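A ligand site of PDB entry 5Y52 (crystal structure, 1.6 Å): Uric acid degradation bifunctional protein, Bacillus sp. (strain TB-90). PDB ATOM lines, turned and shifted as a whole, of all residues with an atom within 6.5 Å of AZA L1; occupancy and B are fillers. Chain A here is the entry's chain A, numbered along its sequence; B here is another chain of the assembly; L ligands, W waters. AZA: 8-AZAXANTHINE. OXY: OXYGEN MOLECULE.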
ATOM      1  N   SER A 182      14.597 -10.345 -29.466  1.00  0.00           N
ATOM      2  CA  SER A 182      15.821  -9.838 -30.063  1.00  0.00           C
ATOM      3  C   SER A 182      15.906  -8.330 -29.897  1.00  0.00           C
ATOM      4  O   SER A 182      14.900  -7.631 -29.769  1.00  0.00           O
ATOM      5  CB  SER A 182      15.909 -10.196 -31.574  1.00  0.00           C
ATOM      6  OG  SER A 182      15.187  -9.291 -32.387  1.00  0.00           O
ATOM      7  N   PHE A 183      17.137  -7.833 -29.897  1.00  0.00           N
ATOM      8  CA  PHE A 183      17.355  -6.400 -29.989  1.00  0.00           C
ATOM      9  C   PHE A 183      18.600  -6.219 -30.851  1.00  0.00           C
ATOM     10  O   PHE A 183      19.729  -6.334 -30.357  1.00  0.00           O
ATOM     11  CB  PHE A 183      17.492  -5.722 -28.631  1.00  0.00           C
ATOM     12  CG  PHE A 183      17.553  -4.212 -28.737  1.00  0.00           C
ATOM     13  CD1 PHE A 183      16.521  -3.528 -29.376  1.00  0.00           C
ATOM     14  CD2 PHE A 183      18.618  -3.489 -28.229  1.00  0.00           C
ATOM     15  CE1 PHE A 183      16.562  -2.160 -29.498  1.00  0.00           C
ATOM     16  CE2 PHE A 183      18.641  -2.072 -28.363  1.00  0.00           C
ATOM     17  CZ  PHE A 183      17.621  -1.444 -28.993  1.00  0.00           C
ATOM     18  N   PHE A 186      20.191  -1.534 -33.984  1.00  0.00           N
ATOM     19  CA  PHE A 186      20.217  -0.186 -33.450  1.00  0.00           C
ATOM     20  C   PHE A 186      21.522   0.539 -33.813  1.00  0.00           C
ATOM     21  O   PHE A 186      22.476  -0.038 -34.359  1.00  0.00           O
ATOM     22  CB  PHE A 186      19.988  -0.197 -31.933  1.00  0.00           C
ATOM     23  CG  PHE A 186      20.854  -1.177 -31.174  1.00  0.00           C
ATOM     24  CD1 PHE A 186      20.464  -2.492 -30.983  1.00  0.00           C
ATOM     25  CD2 PHE A 186      22.058  -0.747 -30.655  1.00  0.00           C
ATOM     26  CE1 PHE A 186      21.301  -3.391 -30.286  1.00  0.00           C
ATOM     27  CE2 PHE A 186      22.878  -1.603 -29.963  1.00  0.00           C
ATOM     28  CZ  PHE A 186      22.513  -2.937 -29.777  1.00  0.00           C
ATOM     29  N   LEU A 194      26.704  -1.759 -26.280  1.00  0.00           N
ATOM     30  CA  LEU A 194      25.728  -2.846 -26.160  1.00  0.00           C
ATOM     31  C   LEU A 194      25.859  -3.799 -27.340  1.00  0.00           C
ATOM     32  O   LEU A 194      25.660  -3.368 -28.484  1.00  0.00           O
ATOM     33  CB  LEU A 194      24.316  -2.270 -26.127  1.00  0.00           C
ATOM     34  CG  LEU A 194      23.196  -3.294 -25.875  1.00  0.00           C
ATOM     35  CD1 LEU A 194      23.307  -3.916 -24.475  1.00  0.00           C
ATOM     36  CD2 LEU A 194      21.830  -2.664 -26.082  1.00  0.00           C
ATOM     37  N   ARG A 200      17.411 -12.807 -26.135  1.00  0.00           N
ATOM     38  CA  ARG A 200      17.589 -12.256 -24.807  1.00  0.00           C
ATOM     39  C   ARG A 200      16.385 -12.589 -23.955  1.00  0.00           C
ATOM     40  O   ARG A 200      15.265 -12.715 -24.475  1.00  0.00           O
ATOM     41  CB  ARG A 200      17.774 -10.730 -24.843  1.00  0.00           C
ATOM     42  CG  ARG A 200      16.571  -9.956 -25.329  1.00  0.00           C
ATOM     43  CD  ARG A 200      16.855  -8.453 -25.255  1.00  0.00           C
ATOM     44  NE  ARG A 200      15.719  -7.681 -25.707  1.00  0.00           N
ATOM     45  CZ  ARG A 200      15.664  -6.355 -25.668  1.00  0.00           C
ATOM     46  NH1 ARG A 200      16.688  -5.654 -25.189  1.00  0.00           N
ATOM     47  NH2 ARG A 200      14.574  -5.751 -26.105  1.00  0.00           N
ATOM     48  N   LEU A 202      14.075 -11.069 -22.228  1.00  0.00           N
ATOM     49  CA  LEU A 202      13.574  -9.716 -21.994  1.00  0.00           C
ATOM     50  C   LEU A 202      12.725  -9.652 -20.738  1.00  0.00           C
ATOM     51  O   LEU A 202      11.774 -10.420 -20.585  1.00  0.00           O
ATOM     52  CB  LEU A 202      12.757  -9.260 -23.189  1.00  0.00           C
ATOM     53  CG  LEU A 202      12.084  -7.905 -23.041  1.00  0.00           C
ATOM     54  CD1 LEU A 202      13.084  -6.776 -22.837  1.00  0.00           C
ATOM     55  CD2 LEU A 202      11.261  -7.629 -24.280  1.00  0.00           C
ATOM     56  N   LEU A 246      11.106  -7.594 -31.103  1.00  0.00           N
ATOM     57  CA  LEU A 246      12.232  -6.920 -31.741  1.00  0.00           C
ATOM     58  C   LEU A 246      12.766  -5.760 -30.925  1.00  0.00           C
ATOM     59  O   LEU A 246      13.799  -5.185 -31.293  1.00  0.00           O
ATOM     60  CB  LEU A 246      11.832  -6.404 -33.127  1.00  0.00           C
ATOM     61  CG  LEU A 246      11.373  -7.462 -34.135  1.00  0.00           C
ATOM     62  CD1 LEU A 246      10.762  -6.807 -35.375  1.00  0.00           C
ATOM     63  CD2 LEU A 246      12.550  -8.340 -34.511  1.00  0.00           C
ATOM     64  N   SER A 247      12.082  -5.408 -29.829  1.00  0.00           N
ATOM     65  CA  SER A 247      12.386  -4.350 -28.875  1.00  0.00           C
ATOM     66  C   SER A 247      11.205  -4.273 -27.918  1.00  0.00           C
ATOM     67  O   SER A 247      10.155  -4.869 -28.177  1.00  0.00           O
ATOM     68  CB  SER A 247      12.564  -2.985 -29.548  1.00  0.00           C
ATOM     69  OG  SER A 247      11.339  -2.563 -30.149  1.00  0.00           O
ATOM     70  N   ILE A 248      11.347  -3.498 -26.849  1.00  0.00           N
ATOM     71  CA  ILE A 248      10.218  -3.221 -25.965  1.00  0.00           C
ATOM     72  C   ILE A 248       9.208  -2.331 -26.669  1.00  0.00           C
ATOM     73  O   ILE A 248       7.997  -2.531 -26.552  1.00  0.00           O
ATOM     74  CB  ILE A 248      10.698  -2.566 -24.668  1.00  0.00           C
ATOM     75  CG1 ILE A 248      11.549  -3.531 -23.860  1.00  0.00           C
ATOM     76  CG2 ILE A 248       9.499  -2.093 -23.849  1.00  0.00           C
ATOM     77  CD1 ILE A 248      12.229  -2.851 -22.635  1.00  0.00           C
ATOM     78  N   GLN A 249       9.711  -1.332 -27.404  1.00  0.00           N
ATOM     79  CA  GLN A 249       8.872  -0.460 -28.239  1.00  0.00           C
ATOM     80  C   GLN A 249       7.959  -1.281 -29.133  1.00  0.00           C
ATOM     81  O   GLN A 249       6.763  -0.997 -29.273  1.00  0.00           O
ATOM     82  CB  GLN A 249       9.782   0.445 -29.082  1.00  0.00           C
ATOM     83  CG  GLN A 249      10.597   1.508 -28.301  1.00  0.00           C
ATOM     84  CD  GLN A 249      11.989   1.043 -27.883  1.00  0.00           C
ATOM     85  OE1 GLN A 249      12.176  -0.109 -27.485  1.00  0.00           O
ATOM     86  NE2 GLN A 249      12.978   1.945 -27.982  1.00  0.00           N
ATOM     87  N   ASN A 275      13.002  -1.480 -18.885  1.00  0.00           N
ATOM     88  CA  ASN A 275      13.838  -2.635 -19.203  1.00  0.00           C
ATOM     89  C   ASN A 275      14.672  -2.998 -17.974  1.00  0.00           C
ATOM     90  O   ASN A 275      15.474  -2.181 -17.509  1.00  0.00           O
ATOM     91  CB  ASN A 275      14.740  -2.301 -20.379  1.00  0.00           C
ATOM     92  CG  ASN A 275      15.448  -3.502 -20.955  1.00  0.00           C
ATOM     93  OD1 ASN A 275      15.531  -4.561 -20.354  1.00  0.00           O
ATOM     94  ND2 ASN A 275      16.013  -3.314 -22.123  1.00  0.00           N
ATOM     95  N   GLY A 301      16.487   1.253 -18.929  1.00  0.00           N
ATOM     96  CA  GLY A 301      15.792   1.862 -20.049  1.00  0.00           C
ATOM     97  C   GLY A 301      14.304   1.987 -19.810  1.00  0.00           C
ATOM     98  O   GLY A 301      13.694   1.254 -19.024  1.00  0.00           O
ATOM     99  N   PHE A 302      13.668   2.931 -20.506  1.00  0.00           N
ATOM    100  CA  PHE A 302      12.221   3.062 -20.404  1.00  0.00           C
ATOM    101  C   PHE A 302      11.635   3.634 -21.680  1.00  0.00           C
ATOM    102  O   PHE A 302      12.314   4.280 -22.486  1.00  0.00           O
ATOM    103  CB  PHE A 302      11.792   3.923 -19.222  1.00  0.00           C
ATOM    104  CG  PHE A 302      12.217   5.367 -19.313  1.00  0.00           C
ATOM    105  CD1 PHE A 302      11.467   6.297 -20.019  1.00  0.00           C
ATOM    106  CD2 PHE A 302      13.347   5.806 -18.664  1.00  0.00           C
ATOM    107  CE1 PHE A 302      11.877   7.626 -20.072  1.00  0.00           C
ATOM    108  CE2 PHE A 302      13.748   7.109 -18.708  1.00  0.00           C
ATOM    109  CZ  PHE A 302      13.023   8.028 -19.403  1.00  0.00           C
ATOM    110  N   GLN A 303      10.330   3.389 -21.851  1.00  0.00           N
ATOM    111  CA  GLN A 303       9.564   3.816 -23.015  1.00  0.00           C
ATOM    112  C   GLN A 303       8.186   4.283 -22.563  1.00  0.00           C
ATOM    113  O   GLN A 303       7.655   3.840 -21.545  1.00  0.00           O
ATOM    114  CB  GLN A 303       9.386   2.660 -24.059  1.00  0.00           C
ATOM    115  CG  GLN A 303      10.681   1.989 -24.603  1.00  0.00           C
ATOM    116  CD  GLN A 303      11.486   1.154 -23.592  1.00  0.00           C
ATOM    117  OE1 GLN A 303      10.957   0.550 -22.642  1.00  0.00           O
ATOM    118  NE2 GLN A 303      12.803   1.079 -23.824  1.00  0.00           N
ATOM    119  N   TYR B  10      11.336   7.785 -25.174  1.00  0.00           N
ATOM    120  CA  TYR B  10      12.012   6.695 -24.496  1.00  0.00           C
ATOM    121  C   TYR B  10      13.324   7.232 -23.953  1.00  0.00           C
ATOM    122  O   TYR B  10      13.781   8.329 -24.338  1.00  0.00           O
ATOM    123  CB  TYR B  10      12.188   5.503 -25.454  1.00  0.00           C
ATOM    124  CG  TYR B  10      13.342   5.608 -26.432  1.00  0.00           C
ATOM    125  CD1 TYR B  10      13.392   6.590 -27.401  1.00  0.00           C
ATOM    126  CD2 TYR B  10      14.392   4.692 -26.384  1.00  0.00           C
ATOM    127  CE1 TYR B  10      14.453   6.682 -28.284  1.00  0.00           C
ATOM    128  CE2 TYR B  10      15.454   4.778 -27.258  1.00  0.00           C
ATOM    129  CZ  TYR B  10      15.498   5.765 -28.199  1.00  0.00           C
ATOM    130  OH  TYR B  10      16.567   5.888 -29.075  1.00  0.00           O
ATOM    131  N   LYS B  12      16.504   6.690 -20.500  1.00  0.00           N
ATOM    132  CA  LYS B  12      17.300   5.953 -19.507  1.00  0.00           C
ATOM    133  C   LYS B  12      17.176   6.684 -18.194  1.00  0.00           C
ATOM    134  O   LYS B  12      17.330   7.916 -18.162  1.00  0.00           O
ATOM    135  CB  LYS B  12      18.766   5.879 -19.927  1.00  0.00           C
ATOM    136  CG  LYS B  12      19.625   4.826 -19.202  1.00  0.00           C
ATOM    137  CD  LYS B  12      19.265   3.434 -19.661  1.00  0.00           C
ATOM    138  CE  LYS B  12      20.327   2.449 -19.296  1.00  0.00           C
ATOM    139  NZ  LYS B  12      20.016   1.084 -19.807  1.00  0.00           N
ATOM    140  N   ASN B  66      14.831  -0.806 -35.746  1.00  0.00           N
ATOM    141  CA  ASN B  66      15.719  -0.149 -34.785  1.00  0.00           C
ATOM    142  C   ASN B  66      16.755   0.746 -35.478  1.00  0.00           C
ATOM    143  O   ASN B  66      17.708   1.199 -34.821  1.00  0.00           O
ATOM    144  CB  ASN B  66      16.406  -1.202 -33.892  1.00  0.00           C
ATOM    145  CG  ASN B  66      15.411  -1.900 -32.969  1.00  0.00           C
ATOM    146  OD1 ASN B  66      14.546  -1.255 -32.372  1.00  0.00           O
ATOM    147  ND2 ASN B  66      15.502  -3.215 -32.864  1.00  0.00           N
ATOM    148  N   VAL B  69      17.150   4.019 -33.656  1.00  0.00           N
ATOM    149  CA  VAL B  69      17.153   3.894 -32.201  1.00  0.00           C
ATOM    150  C   VAL B  69      18.577   4.054 -31.685  1.00  0.00           C
ATOM    151  O   VAL B  69      19.443   3.225 -31.965  1.00  0.00           O
ATOM    152  CB  VAL B  69      16.559   2.549 -31.757  1.00  0.00           C
ATOM    153  CG1 VAL B  69      16.658   2.429 -30.245  1.00  0.00           C
ATOM    154  CG2 VAL B  69      15.121   2.465 -32.209  1.00  0.00           C
ATOM    155  N   VAL B  70      18.795   5.118 -30.939  1.00  0.00           N
ATOM    156  CA  VAL B  70      19.937   5.209 -30.047  1.00  0.00           C
ATOM    157  C   VAL B  70      19.627   4.303 -28.867  1.00  0.00           C
ATOM    158  O   VAL B  70      18.610   4.483 -28.191  1.00  0.00           O
ATOM    159  CB  VAL B  70      20.166   6.666 -29.592  1.00  0.00           C
ATOM    160  CG1 VAL B  70      21.339   6.765 -28.629  1.00  0.00           C
ATOM    161  CG2 VAL B  70      20.417   7.570 -30.786  1.00  0.00           C
ATOM    162  N   ALA B  71      20.481   3.311 -28.622  1.00  0.00           N
ATOM    163  CA  ALA B  71      20.186   2.419 -27.521  1.00  0.00           C
ATOM    164  C   ALA B  71      20.181   3.195 -26.215  1.00  0.00           C
ATOM    165  O   ALA B  71      20.961   4.138 -26.026  1.00  0.00           O
ATOM    166  CB  ALA B  71      21.202   1.276 -27.431  1.00  0.00           C
ATOM    167  N   THR B  72      19.300   2.794 -25.303  1.00  0.00           N
ATOM    168  CA  THR B  72      19.269   3.493 -24.018  1.00  0.00           C
ATOM    169  C   THR B  72      20.571   3.250 -23.267  1.00  0.00           C
ATOM    170  O   THR B  72      21.040   4.128 -22.549  1.00  0.00           O
ATOM    171  CB  THR B  72      18.057   3.058 -23.195  1.00  0.00           C
ATOM    172  OG1 THR B  72      18.189   1.685 -22.845  1.00  0.00           O
ATOM    173  CG2 THR B  72      16.754   3.294 -23.962  1.00  0.00           C
ATOM    174  N   ASP B  73      21.166   2.073 -23.454  1.00  0.00           N
ATOM    175  CA  ASP B  73      22.494   1.826 -22.904  1.00  0.00           C
ATOM    176  C   ASP B  73      23.514   2.846 -23.405  1.00  0.00           C
ATOM    177  O   ASP B  73      24.381   3.287 -22.640  1.00  0.00           O
ATOM    178  CB  ASP B  73      22.900   0.384 -23.249  1.00  0.00           C
ATOM    179  CG  ASP B  73      24.189  -0.017 -22.599  1.00  0.00           C
ATOM    180  OD1 ASP B  73      24.167  -0.426 -21.419  1.00  0.00           O
ATOM    181  OD2 ASP B  73      25.235   0.099 -23.257  1.00  0.00           O
ATOM    182  N   SER B  74      23.433   3.235 -24.684  1.00  0.00           N
ATOM    183  CA  SER B  74      24.311   4.251 -25.255  1.00  0.00           C
ATOM    184  C   SER B  74      24.041   5.610 -24.653  1.00  0.00           C
ATOM    185  O   SER B  74      24.964   6.419 -24.508  1.00  0.00           O
ATOM    186  CB  SER B  74      24.127   4.293 -26.776  1.00  0.00           C
ATOM    187  OG  SER B  74      24.328   2.989 -27.352  1.00  0.00           O
HETATM  188  N1  AZA L   1      14.783  -0.922 -26.464  1.00  0.00           N
HETATM  189  C2  AZA L   1      14.963  -2.193 -26.034  1.00  0.00           C
HETATM  190  O2  AZA L   1      14.073  -2.969 -26.104  1.00  0.00           O
HETATM  191  N3  AZA L   1      16.150  -2.537 -25.531  1.00  0.00           N
HETATM  192  C4  AZA L   1      17.176  -1.712 -25.421  1.00  0.00           C
HETATM  193  C5  AZA L   1      17.001  -0.428 -25.856  1.00  0.00           C
HETATM  194  C6  AZA L   1      15.781  -0.044 -26.387  1.00  0.00           C
HETATM  195  O6  AZA L   1      15.574   1.067 -26.782  1.00  0.00           O
HETATM  196  N7  AZA L   1      18.179   0.190 -25.681  1.00  0.00           N
HETATM  197  N8  AZA L   1      19.077  -0.662 -25.124  1.00  0.00           N
HETATM  198  N9  AZA L   1      18.440  -1.857 -24.973  1.00  0.00           N
HETATM  199  O1  OXY L   2      16.009  -0.199 -22.913  1.00  0.00           O
HETATM  200  O2  OXY L   2      14.958  -0.068 -22.892  1.00  0.00           O
HETATM  201  O   HOH W   1      19.269  -4.301 -23.624  1.00  0.00           O
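Water W1 bridges N9 of AZA L1 and NH1 of Arg 200.
O of Val 70 of chain B sits at hydrogen-bond distance from OH of Tyr 10 of chain B (2.6 Å).
The backbone NH (N) of Asn 275 lies within hydrogen-bond range of the backbone carbonyl oxygen (O) of Gly 301 (2.8 Å).
N of Gln 249 lies close to OG of Ser 247 (3.4 Å).
Merely in contact with AZA L1: Phe 183 (3.3 Å), Ala 71 of chain B (3.5 Å), Ser 247 (3.5 Å), Leu 194 (3.5 Å), Tyr 10 of chain B (3.7 Å), Asp 73 of chain B (3.8 Å), Gln 303 (3.9 Å) and Val 69 of chain B (3.9 Å).
Hydrophobic or aromatic side chains within 4 Å of AZA L1: Phe 183, Leu 194, Ile 248, Tyr 10 of chain B, Val 69 of chain B and Ala 71 of chain B.
13 residues have an atom within 4 Å of AZA L1: Phe 183, Leu 194, Arg 200, Ser 247, Ile 248, Gln 249, Asn 275, Gln 303, Tyr 10 of chain B, Val 69 of chain B, Ala 71 of chain B, Thr 72 of chain B and Asp 73 of chain B.
The nearest printed residue that does not touch AZA L1 is Val 70 of chain B (4.8 Å).
A nitrogen (N3) of AZA L1 sits close to the side-chain amide nitrogen (ND2) of Asn 275 (3.5 Å).
The side-chain amide nitrogen of Gln 303 is in hydrogen-bond range of an oxygen (O2) of OXY L2.
OG1 of Thr 72 of chain B is in hydrogen-bond range of N7 of AZA L1, at 3.2 Å.
The side-chain amide oxygen (OE1) of Gln 249 is in hydrogen-bond range of a nitrogen (N1) of AZA L1 (2.9 Å).
An oxygen (O2) of AZA L1 lies within hydrogen-bond range of the guanidinium group of Arg 200.
The side-chain hydroxyl of Thr 72 of chain B sits at hydrogen-bond distance from an oxygen (O1) of OXY L2 (2.9 Å).
A nitrogen (N7) of AZA L1 sits at hydrogen-bond distance from the backbone NH of Thr 72 of chain B, at 2.9 Å.
The backbone NH of Ile 248 is in hydrogen-bond range of an oxygen (O2) of AZA L1 (2.9 Å).
An oxygen (O1) of OXY L2 is in hydrogen-bond range of the side-chain amide nitrogen of Asn 275, at 3.2 Å.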
